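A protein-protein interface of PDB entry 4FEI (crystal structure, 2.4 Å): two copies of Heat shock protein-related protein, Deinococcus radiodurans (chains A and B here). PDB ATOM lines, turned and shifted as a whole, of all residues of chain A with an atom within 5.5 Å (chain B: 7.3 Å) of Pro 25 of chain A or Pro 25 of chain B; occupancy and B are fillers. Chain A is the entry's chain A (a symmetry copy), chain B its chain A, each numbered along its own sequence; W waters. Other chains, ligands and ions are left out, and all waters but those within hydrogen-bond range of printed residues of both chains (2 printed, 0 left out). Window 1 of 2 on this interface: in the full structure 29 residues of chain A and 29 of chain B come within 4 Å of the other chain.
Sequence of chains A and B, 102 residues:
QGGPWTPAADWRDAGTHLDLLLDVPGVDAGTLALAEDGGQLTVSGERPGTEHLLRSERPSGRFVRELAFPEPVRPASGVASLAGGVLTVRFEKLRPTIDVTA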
ATOM      1  N   TRP A   5      -2.325 -20.632 -39.910  1.00  0.00           N
ATOM      2  CA  TRP A   5      -1.021 -21.000 -39.380  1.00  0.00           C
ATOM      3  C   TRP A   5       0.014 -21.206 -40.488  1.00  0.00           C
ATOM      4  O   TRP A   5      -0.172 -22.051 -41.391  1.00  0.00           O
ATOM      5  CB  TRP A   5      -1.155 -22.299 -38.557  1.00  0.00           C
ATOM      6  CG  TRP A   5       0.001 -22.562 -37.685  1.00  0.00           C
ATOM      7  CD1 TRP A   5       1.010 -21.682 -37.354  1.00  0.00           C
ATOM      8  CD2 TRP A   5       0.269 -23.778 -36.963  1.00  0.00           C
ATOM      9  NE1 TRP A   5       1.879 -22.282 -36.471  1.00  0.00           N
ATOM     10  CE2 TRP A   5       1.445 -23.568 -36.218  1.00  0.00           C
ATOM     11  CE3 TRP A   5      -0.381 -25.024 -36.874  1.00  0.00           C
ATOM     12  CZ2 TRP A   5       1.993 -24.557 -35.403  1.00  0.00           C
ATOM     13  CZ3 TRP A   5       0.165 -25.999 -36.079  1.00  0.00           C
ATOM     14  CH2 TRP A   5       1.352 -25.762 -35.349  1.00  0.00           C
ATOM     15  N   ASP A  23       8.987 -24.371 -36.278  1.00  0.00           N
ATOM     16  CA  ASP A  23       8.327 -24.092 -34.996  1.00  0.00           C
ATOM     17  C   ASP A  23       6.865 -24.562 -35.072  1.00  0.00           C
ATOM     18  O   ASP A  23       6.011 -23.884 -35.689  1.00  0.00           O
ATOM     19  CB  ASP A  23       8.347 -22.593 -34.654  1.00  0.00           C
ATOM     20  CG  ASP A  23       9.685 -22.125 -34.170  1.00  0.00           C
ATOM     21  OD1 ASP A  23       9.947 -20.890 -34.252  1.00  0.00           O
ATOM     22  OD2 ASP A  23      10.475 -22.950 -33.686  1.00  0.00           O
ATOM     23  N   VAL A  24       6.601 -25.718 -34.438  1.00  0.00           N
ATOM     24  CA  VAL A  24       5.257 -26.285 -34.436  1.00  0.00           C
ATOM     25  C   VAL A  24       4.738 -26.582 -32.984  1.00  0.00           C
ATOM     26  O   VAL A  24       4.487 -27.735 -32.631  1.00  0.00           O
ATOM     27  CB  VAL A  24       5.176 -27.558 -35.379  1.00  0.00           C
ATOM     28  CG1 VAL A  24       5.243 -27.165 -36.891  1.00  0.00           C
ATOM     29  CG2 VAL A  24       6.268 -28.564 -35.044  1.00  0.00           C
ATOM     30  N   PRO A  25       4.619 -25.551 -32.131  1.00  0.00           N
ATOM     31  CA  PRO A  25       4.147 -25.853 -30.769  1.00  0.00           C
ATOM     32  C   PRO A  25       2.679 -26.280 -30.749  1.00  0.00           C
ATOM     33  O   PRO A  25       1.886 -25.721 -31.498  1.00  0.00           O
ATOM     34  CB  PRO A  25       4.337 -24.512 -30.014  1.00  0.00           C
ATOM     35  CG  PRO A  25       4.230 -23.497 -31.040  1.00  0.00           C
ATOM     36  CD  PRO A  25       4.831 -24.104 -32.315  1.00  0.00           C
ATOM     37  N   GLY A  26       2.350 -27.281 -29.926  1.00  0.00           N
ATOM     38  CA  GLY A  26       0.961 -27.718 -29.718  1.00  0.00           C
ATOM     39  C   GLY A  26       0.391 -28.590 -30.854  1.00  0.00           C
ATOM     40  O   GLY A  26      -0.804 -28.914 -30.843  1.00  0.00           O
ATOM     41  N   VAL A  27       1.233 -28.988 -31.819  1.00  0.00           N
ATOM     42  CA  VAL A  27       0.777 -29.779 -32.964  1.00  0.00           C
ATOM     43  C   VAL A  27       0.279 -31.155 -32.505  1.00  0.00           C
ATOM     44  O   VAL A  27       0.809 -31.707 -31.525  1.00  0.00           O
ATOM     45  CB  VAL A  27       1.911 -29.920 -33.998  1.00  0.00           C
ATOM     46  CG1 VAL A  27       1.449 -30.529 -35.314  1.00  0.00           C
ATOM     47  CG2 VAL A  27       2.326 -28.615 -34.302  1.00  0.00           C
ATOM     48  N   ARG A  47      -2.951 -28.186 -35.669  1.00  0.00           N
ATOM     49  CA  ARG A  47      -3.202 -28.079 -34.243  1.00  0.00           C
ATOM     50  C   ARG A  47      -4.640 -27.607 -33.985  1.00  0.00           C
ATOM     51  O   ARG A  47      -5.162 -26.796 -34.741  1.00  0.00           O
ATOM     52  CB  ARG A  47      -2.142 -27.235 -33.505  1.00  0.00           C
ATOM     53  CG  ARG A  47      -2.312 -25.736 -33.569  1.00  0.00           C
ATOM     54  CD  ARG A  47      -1.350 -25.108 -32.554  1.00  0.00           C
ATOM     55  NE  ARG A  47      -1.192 -23.666 -32.658  1.00  0.00           N
ATOM     56  CZ  ARG A  47      -0.353 -22.949 -31.901  1.00  0.00           C
ATOM     57  NH1 ARG A  47       0.369 -23.537 -30.951  1.00  0.00           N
ATOM     58  NH2 ARG A  47      -0.271 -21.622 -32.038  1.00  0.00           N
ATOM     59  N   GLY A  84       9.892 -30.409 -27.846  1.00  0.00           N
ATOM     60  CA  GLY A  84       9.695 -29.056 -27.346  1.00  0.00           C
ATOM     61  C   GLY A  84       9.036 -28.082 -28.318  1.00  0.00           C
ATOM     62  O   GLY A  84       9.385 -26.915 -28.340  1.00  0.00           O
ATOM     63  N   GLY A  85       8.084 -28.569 -29.109  1.00  0.00           N
ATOM     64  CA  GLY A  85       7.380 -27.751 -30.085  1.00  0.00           C
ATOM     65  C   GLY A  85       8.199 -27.420 -31.322  1.00  0.00           C
ATOM     66  O   GLY A  85       7.813 -26.577 -32.108  1.00  0.00           O
ATOM     67  N   VAL A  86       9.329 -28.102 -31.509  1.00  0.00           N
ATOM     68  CA  VAL A  86      10.199 -27.864 -32.668  1.00  0.00           C
ATOM     69  C   VAL A  86      10.374 -29.153 -33.476  1.00  0.00           C
ATOM     70  O   VAL A  86      10.826 -30.182 -32.942  1.00  0.00           O
ATOM     71  CB  VAL A  86      11.588 -27.309 -32.208  1.00  0.00           C
ATOM     72  CG1 VAL A  86      12.617 -27.206 -33.369  1.00  0.00           C
ATOM     73  CG2 VAL A  86      11.415 -25.960 -31.434  1.00  0.00           C
ATOM     74  N   TRP B   5      11.994 -11.899 -30.551  1.00  0.00           N
ATOM     75  CA  TRP B   5      10.942 -12.853 -30.233  1.00  0.00           C
ATOM     76  C   TRP B   5       9.826 -12.224 -29.396  1.00  0.00           C
ATOM     77  O   TRP B   5      10.073 -11.698 -28.288  1.00  0.00           O
ATOM     78  CB  TRP B   5      11.552 -14.043 -29.462  1.00  0.00           C
ATOM     79  CG  TRP B   5      10.671 -15.221 -29.410  1.00  0.00           C
ATOM     80  CD1 TRP B   5       9.537 -15.444 -30.162  1.00  0.00           C
ATOM     81  CD2 TRP B   5      10.861 -16.396 -28.601  1.00  0.00           C
ATOM     82  NE1 TRP B   5       9.020 -16.685 -29.866  1.00  0.00           N
ATOM     83  CE2 TRP B   5       9.814 -17.286 -28.910  1.00  0.00           C
ATOM     84  CE3 TRP B   5      11.822 -16.779 -27.646  1.00  0.00           C
ATOM     85  CZ2 TRP B   5       9.693 -18.531 -28.293  1.00  0.00           C
ATOM     86  CZ3 TRP B   5      11.695 -18.000 -27.034  1.00  0.00           C
ATOM     87  CH2 TRP B   5      10.629 -18.869 -27.359  1.00  0.00           C
ATOM     88  N   PRO B   7       6.430 -14.084 -28.368  1.00  0.00           N
ATOM     89  CA  PRO B   7       5.630 -15.320 -28.466  1.00  0.00           C
ATOM     90  C   PRO B   7       4.146 -15.023 -28.394  1.00  0.00           C
ATOM     91  O   PRO B   7       3.705 -14.271 -27.506  1.00  0.00           O
ATOM     92  CB  PRO B   7       6.097 -16.162 -27.260  1.00  0.00           C
ATOM     93  CG  PRO B   7       6.851 -15.245 -26.355  1.00  0.00           C
ATOM     94  CD  PRO B   7       7.281 -14.035 -27.153  1.00  0.00           C
ATOM     95  N   LEU B  22       0.788 -19.672 -24.135  1.00  0.00           N
ATOM     96  CA  LEU B  22       1.876 -18.892 -24.750  1.00  0.00           C
ATOM     97  C   LEU B  22       2.752 -19.817 -25.606  1.00  0.00           C
ATOM     98  O   LEU B  22       3.287 -20.783 -25.095  1.00  0.00           O
ATOM     99  CB  LEU B  22       2.698 -18.191 -23.650  1.00  0.00           C
ATOM    100  CG  LEU B  22       3.640 -17.086 -24.102  1.00  0.00           C
ATOM    101  CD1 LEU B  22       2.855 -15.814 -24.473  1.00  0.00           C
ATOM    102  CD2 LEU B  22       4.707 -16.789 -22.993  1.00  0.00           C
ATOM    103  N   ASP B  23       2.855 -19.532 -26.896  1.00  0.00           N
ATOM    104  CA  ASP B  23       3.626 -20.386 -27.810  1.00  0.00           C
ATOM    105  C   ASP B  23       5.124 -20.113 -27.608  1.00  0.00           C
ATOM    106  O   ASP B  23       5.652 -19.081 -28.086  1.00  0.00           O
ATOM    107  CB  ASP B  23       3.268 -20.121 -29.281  1.00  0.00           C
ATOM    108  CG  ASP B  23       1.956 -20.724 -29.679  1.00  0.00           C
ATOM    109  OD1 ASP B  23       1.367 -20.249 -30.693  1.00  0.00           O
ATOM    110  OD2 ASP B  23       1.506 -21.678 -29.024  1.00  0.00           O
ATOM    111  N   VAL B  24       5.788 -21.046 -26.903  1.00  0.00           N
ATOM    112  CA  VAL B  24       7.215 -20.910 -26.629  1.00  0.00           C
ATOM    113  C   VAL B  24       8.031 -22.172 -27.082  1.00  0.00           C
ATOM    114  O   VAL B  24       8.634 -22.858 -26.256  1.00  0.00           O
ATOM    115  CB  VAL B  24       7.467 -20.539 -25.108  1.00  0.00           C
ATOM    116  CG1 VAL B  24       7.044 -19.068 -24.790  1.00  0.00           C
ATOM    117  CG2 VAL B  24       6.754 -21.509 -24.177  1.00  0.00           C
ATOM    118  N   PRO B  25       8.016 -22.502 -28.385  1.00  0.00           N
ATOM    119  CA  PRO B  25       8.774 -23.698 -28.786  1.00  0.00           C
ATOM    120  C   PRO B  25      10.285 -23.491 -28.665  1.00  0.00           C
ATOM    121  O   PRO B  25      10.763 -22.405 -28.971  1.00  0.00           O
ATOM    122  CB  PRO B  25       8.368 -23.905 -30.268  1.00  0.00           C
ATOM    123  CG  PRO B  25       8.027 -22.580 -30.741  1.00  0.00           C
ATOM    124  CD  PRO B  25       7.402 -21.842 -29.550  1.00  0.00           C
ATOM    125  N   GLY B  26      11.001 -24.516 -28.190  1.00  0.00           N
ATOM    126  CA  GLY B  26      12.470 -24.500 -28.129  1.00  0.00           C
ATOM    127  C   GLY B  26      13.049 -23.677 -26.961  1.00  0.00           C
ATOM    128  O   GLY B  26      14.272 -23.494 -26.881  1.00  0.00           O
ATOM    129  N   VAL B  27      12.191 -23.197 -26.049  1.00  0.00           N
ATOM    130  CA  VAL B  27      12.640 -22.364 -24.930  1.00  0.00           C
ATOM    131  C   VAL B  27      13.554 -23.166 -23.995  1.00  0.00           C
ATOM    132  O   VAL B  27      13.362 -24.384 -23.840  1.00  0.00           O
ATOM    133  CB  VAL B  27      11.425 -21.803 -24.167  1.00  0.00           C
ATOM    134  CG1 VAL B  27      11.802 -20.748 -23.136  1.00  0.00           C
ATOM    135  CG2 VAL B  27      10.635 -21.144 -25.120  1.00  0.00           C
ATOM    136  N   ASP B  28      14.561 -22.495 -23.441  1.00  0.00           N
ATOM    137  CA  ASP B  28      15.328 -23.036 -22.340  1.00  0.00           C
ATOM    138  C   ASP B  28      14.378 -22.910 -21.137  1.00  0.00           C
ATOM    139  O   ASP B  28      14.070 -21.782 -20.683  1.00  0.00           O
ATOM    140  CB  ASP B  28      16.590 -22.193 -22.106  1.00  0.00           C
ATOM    141  CG  ASP B  28      17.470 -22.744 -20.970  1.00  0.00           C
ATOM    142  OD1 ASP B  28      17.011 -23.578 -20.111  1.00  0.00           O
ATOM    143  OD2 ASP B  28      18.663 -22.345 -20.936  1.00  0.00           O
ATOM    144  N   GLU B  46      13.871 -17.274 -22.689  1.00  0.00           N
ATOM    145  CA  GLU B  46      14.878 -17.199 -23.718  1.00  0.00           C
ATOM    146  C   GLU B  46      14.938 -18.489 -24.525  1.00  0.00           C
ATOM    147  O   GLU B  46      14.684 -19.574 -24.000  1.00  0.00           O
ATOM    148  CB  GLU B  46      16.228 -16.950 -23.046  1.00  0.00           C
ATOM    149  CG  GLU B  46      17.409 -16.802 -23.988  1.00  0.00           C
ATOM    150  CD  GLU B  46      18.729 -16.609 -23.273  1.00  0.00           C
ATOM    151  OE1 GLU B  46      19.774 -16.389 -23.953  1.00  0.00           O
ATOM    152  OE2 GLU B  46      18.745 -16.681 -22.045  1.00  0.00           O
ATOM    153  N   ARG B  47      15.301 -18.376 -25.802  1.00  0.00           N
ATOM    154  CA  ARG B  47      15.753 -19.531 -26.556  1.00  0.00           C
ATOM    155  C   ARG B  47      17.037 -19.199 -27.329  1.00  0.00           C
ATOM    156  O   ARG B  47      17.190 -18.082 -27.808  1.00  0.00           O
ATOM    157  CB  ARG B  47      14.648 -20.141 -27.443  1.00  0.00           C
ATOM    158  CG  ARG B  47      14.403 -19.468 -28.772  1.00  0.00           C
ATOM    159  CD  ARG B  47      13.495 -20.381 -29.604  1.00  0.00           C
ATOM    160  NE  ARG B  47      12.947 -19.780 -30.810  1.00  0.00           N
ATOM    161  CZ  ARG B  47      12.089 -20.397 -31.630  1.00  0.00           C
ATOM    162  NH1 ARG B  47      11.719 -21.654 -31.398  1.00  0.00           N
ATOM    163  NH2 ARG B  47      11.638 -19.790 -32.732  1.00  0.00           N
ATOM    164  N   ARG B  58      12.649 -17.892 -38.104  1.00  0.00           N
ATOM    165  CA  ARG B  58      12.324 -18.134 -36.713  1.00  0.00           C
ATOM    166  C   ARG B  58      12.955 -17.103 -35.801  1.00  0.00           C
ATOM    167  O   ARG B  58      14.125 -16.754 -35.981  1.00  0.00           O
ATOM    168  CB  ARG B  58      12.812 -19.523 -36.302  1.00  0.00           C
ATOM    169  CG  ARG B  58      12.154 -20.721 -37.065  1.00  0.00           C
ATOM    170  CD  ARG B  58      12.310 -22.000 -36.277  1.00  0.00           C
ATOM    171  NE  ARG B  58      13.678 -22.081 -35.769  1.00  0.00           N
ATOM    172  CZ  ARG B  58      14.053 -22.733 -34.672  1.00  0.00           C
ATOM    173  NH1 ARG B  58      15.338 -22.724 -34.324  1.00  0.00           N
ATOM    174  NH2 ARG B  58      13.161 -23.393 -33.932  1.00  0.00           N
ATOM    175  N   PRO B  59      12.191 -16.623 -34.785  1.00  0.00           N
ATOM    176  CA  PRO B  59      12.740 -15.687 -33.772  1.00  0.00           C
ATOM    177  C   PRO B  59      13.704 -16.361 -32.790  1.00  0.00           C
ATOM    178  O   PRO B  59      13.535 -17.546 -32.509  1.00  0.00           O
ATOM    179  CB  PRO B  59      11.500 -15.230 -32.997  1.00  0.00           C
ATOM    180  CG  PRO B  59      10.306 -15.921 -33.598  1.00  0.00           C
ATOM    181  CD  PRO B  59      10.793 -17.015 -34.484  1.00  0.00           C
ATOM    182  N   LEU B  82       4.421 -26.464 -18.827  1.00  0.00           N
ATOM    183  CA  LEU B  82       4.996 -26.400 -20.178  1.00  0.00           C
ATOM    184  C   LEU B  82       5.003 -27.774 -20.817  1.00  0.00           C
ATOM    185  O   LEU B  82       5.560 -28.708 -20.254  1.00  0.00           O
ATOM    186  CB  LEU B  82       6.432 -25.903 -20.136  1.00  0.00           C
ATOM    187  CG  LEU B  82       7.247 -25.914 -21.456  1.00  0.00           C
ATOM    188  CD1 LEU B  82       6.884 -24.721 -22.348  1.00  0.00           C
ATOM    189  CD2 LEU B  82       8.758 -25.963 -21.246  1.00  0.00           C
ATOM    190  N   ALA B  83       4.376 -27.906 -21.980  1.00  0.00           N
ATOM    191  CA  ALA B  83       4.382 -29.161 -22.742  1.00  0.00           C
ATOM    192  C   ALA B  83       4.223 -28.866 -24.234  1.00  0.00           C
ATOM    193  O   ALA B  83       3.394 -28.049 -24.627  1.00  0.00           O
ATOM    194  CB  ALA B  83       3.256 -30.134 -22.265  1.00  0.00           C
ATOM    195  N   GLY B  84       5.018 -29.545 -25.044  1.00  0.00           N
ATOM    196  CA  GLY B  84       4.933 -29.419 -26.491  1.00  0.00           C
ATOM    197  C   GLY B  84       5.136 -28.011 -27.045  1.00  0.00           C
ATOM    198  O   GLY B  84       4.492 -27.639 -28.010  1.00  0.00           O
ATOM    199  N   GLY B  85       6.035 -27.246 -26.433  1.00  0.00           N
ATOM    200  CA  GLY B  85       6.322 -25.883 -26.854  1.00  0.00           C
ATOM    201  C   GLY B  85       5.247 -24.877 -26.473  1.00  0.00           C
ATOM    202  O   GLY B  85       5.258 -23.757 -26.946  1.00  0.00           O
ATOM    203  N   VAL B  86       4.323 -25.271 -25.598  1.00  0.00           N
ATOM    204  CA  VAL B  86       3.238 -24.384 -25.160  1.00  0.00           C
ATOM    205  C   VAL B  86       3.276 -24.207 -23.640  1.00  0.00           C
ATOM    206  O   VAL B  86       3.208 -25.193 -22.882  1.00  0.00           O
ATOM    207  CB  VAL B  86       1.851 -24.946 -25.615  1.00  0.00           C
ATOM    208  CG1 VAL B  86       0.649 -24.151 -25.030  1.00  0.00           C
ATOM    209  CG2 VAL B  86       1.789 -25.070 -27.174  1.00  0.00           C
ATOM    210  N   LEU B  87       3.323 -22.958 -23.196  1.00  0.00           N
ATOM    211  CA  LEU B  87       3.190 -22.651 -21.784  1.00  0.00           C
ATOM    212  C   LEU B  87       1.740 -22.366 -21.407  1.00  0.00           C
ATOM    213  O   LEU B  87       1.149 -21.430 -21.897  1.00  0.00           O
ATOM    214  CB  LEU B  87       4.068 -21.461 -21.429  1.00  0.00           C
ATOM    215  CG  LEU B  87       4.033 -21.013 -19.956  1.00  0.00           C
ATOM    216  CD1 LEU B  87       4.672 -22.042 -19.049  1.00  0.00           C
ATOM    217  CD2 LEU B  87       4.742 -19.703 -19.854  1.00  0.00           C
HETATM  218  O   HOH W   1       9.252 -25.496 -25.308  1.00  0.00           O
HETATM  219  O   HOH W   2       4.758 -29.746 -30.601  1.00  0.00           O
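The backbone NH (N) of Val 24 of chain B is in hydrogen-bond range of the backbone carbonyl oxygen (O) of Gly 85 of chain B (2.8 Å). The guanidinium group (NH1) of Arg 47 of chain B sits at hydrogen-bond distance from the backbone carbonyl oxygen (O) of Pro 25 of chain B (2.7 Å). NE of Arg 47 of chain B sits at hydrogen-bond distance from O of Pro 59 of chain B (2.9 Å). O of Gly 85 of chain A is in hydrogen-bond range of N of Val 24 of chain A. The backbone carbonyl oxygen (O) of Pro 25 of chain A lies within hydrogen-bond range of the guanidinium group (NH1) of Arg 47 of chain A.
Asp 23 of chain A touches Pro 25 of chain B, and with the chains exchanged Pro 25 of chain A touches Asp 23 of chain B. Asp 23 of chain A touches Arg 47 of chain B, and with the chains exchanged Arg 47 of chain A touches Asp 23 of chain B. Pro 25 of chain B touches its own counterpart, Pro 25 of chain A. Gly 26 of chain A touches Gly 84 of chain B, and with the chains exchanged Gly 84 of chain A touches Gly 26 of chain B.
Of chain B, only Asp 23, Pro 25, Gly 84, Gly 85 and Val 86 come within 4 Å of Pro 25 of chain A. Pro 25 of chain B touches just these residues of chain A: Asp 23, Pro 25, Gly 84, Gly 85 and Val 86. Of the printed residues of chain A, Pro 59 of chain B touches Asp 23. Of the printed residues of chain A, Gly 85 of chain B touches Pro 25, Gly 84 and Gly 85. Printed residues of chain A within 4 Å of Arg 58 of chain B: Asp 23 and Val 86. Of the printed residues of chain B, Gly 85 of chain A touches Pro 25, Gly 84 and Gly 85. Leu 87 of chain B touches none of the printed residues of chain A. Val 27 of chain B touches none of the printed residues of chain A. The nearest residue of chain B that does not touch Pro 25 of chain A is Val 24 of chain B (4.9 Å).
Water W2 bridges O of Val 24 of chain A and O of Gly 84 of chain B. Water W1 lies within hydrogen-bond range of the backbone carbonyl oxygen (O) of Val 24 of chain B and the backbone carbonyl oxygen (O) of Gly 84 of chain A.
The side-chain carboxylate of Asp 23 of chain B is in salt-bridge range of the guanidinium group of Arg 47 of chain A (2.5 Å). The backbone carbonyl oxygen of Gly 84 of chain A sits at hydrogen-bond distance from the backbone NH of Gly 26 of chain B. NH2 of Arg 47 of chain B is in salt-bridge range of OD1 of Asp 23 of chain A. The guanidinium group (NH2) of Arg 58 of chain B is in salt-bridge range of the side-chain carboxylate (OD2) of Asp 23 of chain A, at 2.7 Å. The backbone NH (N) of Gly 26 of chain A lies within hydrogen-bond range of the backbone carbonyl oxygen (O) of Gly 84 of chain B (2.9 Å).
Of the 19 printed residues of chain B, 9 touch a printed residue of chain A. Hydrophobic or aromatic side chains of chain B that line the printed part of chain A: Pro 25, Pro 59 and Val 86.
Among the printed residues, pairs that only touch across the chains: Pro 25 of chain A with Gly 85 of chain B (3.3 Å), Gly 85 of chain A with Pro 25 of chain B (3.3 Å), Pro 25 of chain A with Gly 84 of chain B (3.3 Å), Gly 84 of chain A with Pro 25 of chain B (3.3 Å), Gly 84 of chain A with Gly 85 of chain B (3.6 Å), Gly 85 of chain A with Gly 84 of chain B (3.6 Å), Gly 26 of chain A with Val 86 of chain B (3.6 Å), Val 86 of chain A with Gly 26 of chain B (3.6 Å), Gly 85 of chain A with Gly 85 of chain B (3.6 Å), Pro 25 of chain A with Asp 23 of chain B (3.8 Å), Asp 23 of chain A with Pro 25 of chain B (3.8 Å), Val 86 of chain A with Pro 25 of chain B (3.9 Å), Pro 25 of chain A with Val 86 of chain B (3.9 Å), Pro 25 of chain A with Pro 25 of chain B (3.9 Å), Val 86 of chain A with Arg 58 of chain B (3.9 Å) and Asp 23 of chain A with Pro 59 of chain B (3.97 Å).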
